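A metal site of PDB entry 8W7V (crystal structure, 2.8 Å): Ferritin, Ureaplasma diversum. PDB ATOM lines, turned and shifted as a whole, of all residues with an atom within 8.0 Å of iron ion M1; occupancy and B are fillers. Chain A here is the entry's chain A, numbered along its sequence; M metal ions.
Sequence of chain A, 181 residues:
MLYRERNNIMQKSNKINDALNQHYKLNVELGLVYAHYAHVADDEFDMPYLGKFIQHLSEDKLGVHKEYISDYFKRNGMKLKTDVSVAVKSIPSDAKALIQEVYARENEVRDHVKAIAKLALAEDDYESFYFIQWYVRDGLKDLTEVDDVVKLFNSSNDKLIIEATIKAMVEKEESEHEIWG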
ATOM      1  N   ASN A  27      33.623  11.753   2.645  1.00  0.00           N
ATOM      2  CA  ASN A  27      32.803  10.636   2.992  1.00  0.00           C
ATOM      3  C   ASN A  27      32.820   9.549   1.972  1.00  0.00           C
ATOM      4  O   ASN A  27      32.808   8.391   2.301  1.00  0.00           O
ATOM      5  CB  ASN A  27      31.396  11.137   3.278  1.00  0.00           C
ATOM      6  CG  ASN A  27      31.257  11.760   4.637  1.00  0.00           C
ATOM      7  OD1 ASN A  27      31.452  11.117   5.650  1.00  0.00           O
ATOM      8  ND2 ASN A  27      30.885  13.011   4.664  1.00  0.00           N
ATOM      9  N   HIS A  56      30.015  -1.462   8.067  1.00  0.00           N
ATOM     10  CA  HIS A  56      28.883  -0.660   8.415  1.00  0.00           C
ATOM     11  C   HIS A  56      29.206   0.807   8.438  1.00  0.00           C
ATOM     12  O   HIS A  56      28.351   1.612   8.204  1.00  0.00           O
ATOM     13  CB  HIS A  56      28.271  -1.134   9.704  1.00  0.00           C
ATOM     14  CG  HIS A  56      27.568  -2.457   9.597  1.00  0.00           C
ATOM     15  ND1 HIS A  56      27.618  -3.245   8.475  1.00  0.00           N
ATOM     16  CD2 HIS A  56      26.818  -3.138  10.492  1.00  0.00           C
ATOM     17  CE1 HIS A  56      26.918  -4.354   8.677  1.00  0.00           C
ATOM     18  NE2 HIS A  56      26.426  -4.307   9.895  1.00  0.00           N
ATOM     19  N   LEU A  57      30.446   1.155   8.679  1.00  0.00           N
ATOM     20  CA  LEU A  57      30.875   2.519   8.623  1.00  0.00           C
ATOM     21  C   LEU A  57      31.042   2.984   7.214  1.00  0.00           C
ATOM     22  O   LEU A  57      30.792   4.108   6.920  1.00  0.00           O
ATOM     23  CB  LEU A  57      32.197   2.643   9.319  1.00  0.00           C
ATOM     24  CG  LEU A  57      32.335   3.290  10.676  1.00  0.00           C
ATOM     25  CD1 LEU A  57      33.796   3.215  11.016  1.00  0.00           C
ATOM     26  CD2 LEU A  57      31.873   4.743  10.644  1.00  0.00           C
ATOM     27  N   GLU A  59      29.343   2.023   4.760  1.00  0.00           N
ATOM     28  CA  GLU A  59      28.055   2.180   4.214  1.00  0.00           C
ATOM     29  C   GLU A  59      27.318   3.369   4.749  1.00  0.00           C
ATOM     30  O   GLU A  59      26.405   3.842   4.121  1.00  0.00           O
ATOM     31  CB  GLU A  59      27.323   0.895   4.468  1.00  0.00           C
ATOM     32  CG  GLU A  59      27.704  -0.252   3.565  1.00  0.00           C
ATOM     33  CD  GLU A  59      27.252  -1.589   4.101  1.00  0.00           C
ATOM     34  OE1 GLU A  59      27.441  -2.602   3.408  1.00  0.00           O
ATOM     35  OE2 GLU A  59      26.718  -1.649   5.218  1.00  0.00           O
ATOM     36  N   ASP A  60      27.733   3.890   5.881  1.00  0.00           N
ATOM     37  CA  ASP A  60      27.148   5.060   6.471  1.00  0.00           C
ATOM     38  C   ASP A  60      27.689   6.247   5.781  1.00  0.00           C
ATOM     39  O   ASP A  60      26.994   7.179   5.520  1.00  0.00           O
ATOM     40  CB  ASP A  60      27.565   5.053   7.933  1.00  0.00           C
ATOM     41  CG  ASP A  60      26.861   6.050   8.762  1.00  0.00           C
ATOM     42  OD1 ASP A  60      25.622   6.109   8.694  1.00  0.00           O
ATOM     43  OD2 ASP A  60      27.543   6.769   9.526  1.00  0.00           O
ATOM     44  N   LYS A  61      28.952   6.213   5.469  1.00  0.00           N
ATOM     45  CA  LYS A  61      29.611   7.315   4.852  1.00  0.00           C
ATOM     46  C   LYS A  61      29.284   7.435   3.404  1.00  0.00           C
ATOM     47  O   LYS A  61      29.107   8.514   2.891  1.00  0.00           O
ATOM     48  CB  LYS A  61      31.107   7.125   5.013  1.00  0.00           C
ATOM     49  CG  LYS A  61      31.734   7.141   6.395  1.00  0.00           C
ATOM     50  CD  LYS A  61      31.084   8.108   7.363  1.00  0.00           C
ATOM     51  CE  LYS A  61      31.958   8.346   8.581  1.00  0.00           C
ATOM     52  NZ  LYS A  61      32.160   9.800   8.809  1.00  0.00           N
ATOM     53  N   VAL A  64      24.219   7.846   3.893  1.00  0.00           N
ATOM     54  CA  VAL A  64      23.519   9.013   4.395  1.00  0.00           C
ATOM     55  C   VAL A  64      24.344  10.244   4.548  1.00  0.00           C
ATOM     56  O   VAL A  64      23.844  11.314   4.390  1.00  0.00           O
ATOM     57  CB  VAL A  64      22.794   8.702   5.693  1.00  0.00           C
ATOM     58  CG1 VAL A  64      21.517   7.942   5.419  1.00  0.00           C
ATOM     59  CG2 VAL A  64      23.677   7.964   6.673  1.00  0.00           C
ATOM     60  N   HIS A  65      25.623  10.102   4.776  1.00  0.00           N
ATOM     61  CA  HIS A  65      26.482  11.216   4.962  1.00  0.00           C
ATOM     62  C   HIS A  65      26.630  11.921   3.662  1.00  0.00           C
ATOM     63  O   HIS A  65      26.769  13.113   3.622  1.00  0.00           O
ATOM     64  CB  HIS A  65      27.807  10.749   5.464  1.00  0.00           C
ATOM     65  CG  HIS A  65      27.846  10.391   6.918  1.00  0.00           C
ATOM     66  ND1 HIS A  65      28.696  11.016   7.811  1.00  0.00           N
ATOM     67  CD2 HIS A  65      27.201   9.447   7.628  1.00  0.00           C
ATOM     68  CE1 HIS A  65      28.540  10.495   9.006  1.00  0.00           C
ATOM     69  NE2 HIS A  65      27.651   9.521   8.929  1.00  0.00           N
ATOM     70  N   GLU A 106      38.246   9.604  11.912  1.00  0.00           N
ATOM     71  CA  GLU A 106      37.007  10.072  12.484  1.00  0.00           C
ATOM     72  C   GLU A 106      37.135  11.307  13.340  1.00  0.00           C
ATOM     73  O   GLU A 106      36.243  12.096  13.401  1.00  0.00           O
ATOM     74  CB  GLU A 106      36.346   8.926  13.269  1.00  0.00           C
ATOM     75  CG  GLU A 106      35.874   7.754  12.452  1.00  0.00           C
ATOM     76  CD  GLU A 106      34.797   8.105  11.463  1.00  0.00           C
ATOM     77  OE1 GLU A 106      33.752   8.634  11.880  1.00  0.00           O
ATOM     78  OE2 GLU A 106      34.989   7.871  10.262  1.00  0.00           O
ATOM     79  N   VAL A 109      37.144  14.068  11.058  1.00  0.00           N
ATOM     80  CA  VAL A 109      35.850  14.418  10.552  1.00  0.00           C
ATOM     81  C   VAL A 109      35.268  15.420  11.484  1.00  0.00           C
ATOM     82  O   VAL A 109      34.702  16.395  11.081  1.00  0.00           O
ATOM     83  CB  VAL A 109      34.950  13.155  10.412  1.00  0.00           C
ATOM     84  CG1 VAL A 109      33.481  13.513  10.229  1.00  0.00           C
ATOM     85  CG2 VAL A 109      35.408  12.264   9.285  1.00  0.00           C
ATOM     86  N   TRP A 134      23.521  17.685  12.457  1.00  0.00           N
ATOM     87  CA  TRP A 134      23.495  16.248  12.377  1.00  0.00           C
ATOM     88  C   TRP A 134      24.880  15.740  12.358  1.00  0.00           C
ATOM     89  O   TRP A 134      25.209  14.759  12.986  1.00  0.00           O
ATOM     90  CB  TRP A 134      22.794  15.829  11.099  1.00  0.00           C
ATOM     91  CG  TRP A 134      22.545  14.369  10.958  1.00  0.00           C
ATOM     92  CD1 TRP A 134      21.465  13.693  11.400  1.00  0.00           C
ATOM     93  CD2 TRP A 134      23.380  13.407  10.294  1.00  0.00           C
ATOM     94  NE1 TRP A 134      21.576  12.364  11.088  1.00  0.00           N
ATOM     95  CE2 TRP A 134      22.746  12.168  10.413  1.00  0.00           C
ATOM     96  CE3 TRP A 134      24.608  13.472   9.646  1.00  0.00           C
ATOM     97  CZ2 TRP A 134      23.296  11.005   9.896  1.00  0.00           C
ATOM     98  CZ3 TRP A 134      25.146  12.324   9.138  1.00  0.00           C
ATOM     99  CH2 TRP A 134      24.491  11.107   9.257  1.00  0.00           C
ATOM    100  N   TYR A 135      25.710  16.423  11.632  1.00  0.00           N
ATOM    101  CA  TYR A 135      27.062  16.009  11.474  1.00  0.00           C
ATOM    102  C   TYR A 135      27.909  16.311  12.682  1.00  0.00           C
ATOM    103  O   TYR A 135      28.880  15.642  12.902  1.00  0.00           O
ATOM    104  CB  TYR A 135      27.577  16.679  10.222  1.00  0.00           C
ATOM    105  CG  TYR A 135      26.981  16.202   8.923  1.00  0.00           C
ATOM    106  CD1 TYR A 135      25.820  16.749   8.424  1.00  0.00           C
ATOM    107  CD2 TYR A 135      27.607  15.230   8.184  1.00  0.00           C
ATOM    108  CE1 TYR A 135      25.282  16.318   7.246  1.00  0.00           C
ATOM    109  CE2 TYR A 135      27.083  14.788   6.988  1.00  0.00           C
ATOM    110  CZ  TYR A 135      25.913  15.341   6.530  1.00  0.00           C
ATOM    111  OH  TYR A 135      25.384  14.904   5.362  1.00  0.00           O
ATOM    112  N   ARG A 137      26.791  16.014  15.682  1.00  0.00           N
ATOM    113  CA  ARG A 137      26.454  14.915  16.529  1.00  0.00           C
ATOM    114  C   ARG A 137      26.970  13.541  16.128  1.00  0.00           C
ATOM    115  O   ARG A 137      27.400  12.791  16.971  1.00  0.00           O
ATOM    116  CB  ARG A 137      24.951  14.922  16.660  1.00  0.00           C
ATOM    117  CG  ARG A 137      24.310  13.780  17.390  1.00  0.00           C
ATOM    118  CD  ARG A 137      22.963  13.397  16.812  1.00  0.00           C
ATOM    119  NE  ARG A 137      22.993  13.085  15.396  1.00  0.00           N
ATOM    120  CZ  ARG A 137      23.423  11.939  14.867  1.00  0.00           C
ATOM    121  NH1 ARG A 137      23.878  10.967  15.628  1.00  0.00           N
ATOM    122  NH2 ARG A 137      23.410  11.769  13.572  1.00  0.00           N
ATOM    123  N   ASP A 138      26.972  13.224  14.853  1.00  0.00           N
ATOM    124  CA  ASP A 138      27.408  11.909  14.390  1.00  0.00           C
ATOM    125  C   ASP A 138      28.885  11.831  14.441  1.00  0.00           C
ATOM    126  O   ASP A 138      29.444  10.770  14.353  1.00  0.00           O
ATOM    127  CB  ASP A 138      26.931  11.650  12.961  1.00  0.00           C
ATOM    128  CG  ASP A 138      26.583  10.233  12.705  1.00  0.00           C
ATOM    129  OD1 ASP A 138      25.640   9.747  13.340  1.00  0.00           O
ATOM    130  OD2 ASP A 138      27.216   9.612  11.837  1.00  0.00           O
ATOM    131  N   GLY A 139      29.529  12.960  14.582  1.00  0.00           N
ATOM    132  CA  GLY A 139      30.940  12.989  14.661  1.00  0.00           C
ATOM    133  C   GLY A 139      31.459  12.406  15.895  1.00  0.00           C
ATOM    134  O   GLY A 139      32.424  11.692  15.880  1.00  0.00           O
ATOM    135  N   LYS A 141      29.546  10.568  17.844  1.00  0.00           N
ATOM    136  CA  LYS A 141      29.009   9.255  17.929  1.00  0.00           C
ATOM    137  C   LYS A 141      29.763   8.187  17.209  1.00  0.00           C
ATOM    138  O   LYS A 141      29.950   7.122  17.721  1.00  0.00           O
ATOM    139  CB  LYS A 141      27.584   9.221  17.454  1.00  0.00           C
ATOM    140  CG  LYS A 141      26.716   8.279  18.259  1.00  0.00           C
ATOM    141  CD  LYS A 141      25.970   7.339  17.344  1.00  0.00           C
ATOM    142  CE  LYS A 141      26.068   7.840  15.922  1.00  0.00           C
ATOM    143  NZ  LYS A 141      26.126   6.759  14.902  1.00  0.00           N
ATOM    144  N   ASP A 142      30.180   8.477  16.023  1.00  0.00           N
ATOM    145  CA  ASP A 142      30.820   7.472  15.263  1.00  0.00           C
ATOM    146  C   ASP A 142      32.189   7.276  15.809  1.00  0.00           C
ATOM    147  O   ASP A 142      32.746   6.232  15.682  1.00  0.00           O
ATOM    148  CB  ASP A 142      30.827   7.846  13.779  1.00  0.00           C
ATOM    149  CG  ASP A 142      29.558   7.473  13.062  1.00  0.00           C
ATOM    150  OD1 ASP A 142      28.701   6.808  13.671  1.00  0.00           O
ATOM    151  OD2 ASP A 142      29.396   7.828  11.870  1.00  0.00           O
ATOM    152  N   LEU A 143      32.740   8.270  16.473  1.00  0.00           N
ATOM    153  CA  LEU A 143      34.032   8.127  17.105  1.00  0.00           C
ATOM    154  C   LEU A 143      33.932   7.371  18.365  1.00  0.00           C
ATOM    155  O   LEU A 143      34.819   6.644  18.701  1.00  0.00           O
ATOM    156  CB  LEU A 143      34.637   9.511  17.350  1.00  0.00           C
ATOM    157  CG  LEU A 143      35.952   9.669  18.083  1.00  0.00           C
ATOM    158  CD1 LEU A 143      37.009  10.142  17.122  1.00  0.00           C
ATOM    159  CD2 LEU A 143      35.806  10.646  19.235  1.00  0.00           C
ATOM    160  N   GLU A 145      31.826   5.028  18.937  1.00  0.00           N
ATOM    161  CA  GLU A 145      31.721   3.664  18.530  1.00  0.00           C
ATOM    162  C   GLU A 145      33.038   3.084  18.181  1.00  0.00           C
ATOM    163  O   GLU A 145      33.361   2.024  18.624  1.00  0.00           O
ATOM    164  CB  GLU A 145      30.810   3.605  17.349  1.00  0.00           C
ATOM    165  CG  GLU A 145      29.338   3.809  17.642  1.00  0.00           C
ATOM    166  CD  GLU A 145      28.517   3.826  16.371  1.00  0.00           C
ATOM    167  OE1 GLU A 145      29.060   3.498  15.297  1.00  0.00           O
ATOM    168  OE2 GLU A 145      27.323   4.149  16.443  1.00  0.00           O
HETATM  169 FE    FE M   1      27.625   8.436  10.528  1.00  0.00          FE
HETATM  170 FE    FE M   2      25.157   3.433  11.851  1.00  0.00          FE
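The side-chain carboxylate (OD1) of Asp 138 lies within salt-bridge range of the side-chain amino group (NZ) of Lys 141 (3.4 Å). The side-chain carboxylate (OD1) of Asp 138 lies within salt-bridge range of the guanidinium group (NH2) of Arg 137, 3.0 Å away. The side-chain hydroxyl of Tyr 135 is in hydrogen-bond range of the backbone carbonyl oxygen of His 65 (2.9 Å). The side-chain carboxylate (OD1) of Asp 142 lies within salt-bridge range of the side-chain amino group (NZ) of Lys 141 (2.9 Å).
The nearest printed residue that does not touch iron ion M1 is Trp 134 (4.3 Å).
OD2 of Asp 138 is bound to iron ion M1 (1.8 Å). NE2 of His 65 binds iron ion M1 (1.9 Å). OD2 of Asp 60 is bound to iron ion M1 (1.9 Å). The side-chain carboxylate (OD2) of Asp 142 is bound to iron ion M1, at 2.3 Å. Iron ion M1 has four donor atoms within binding distance.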
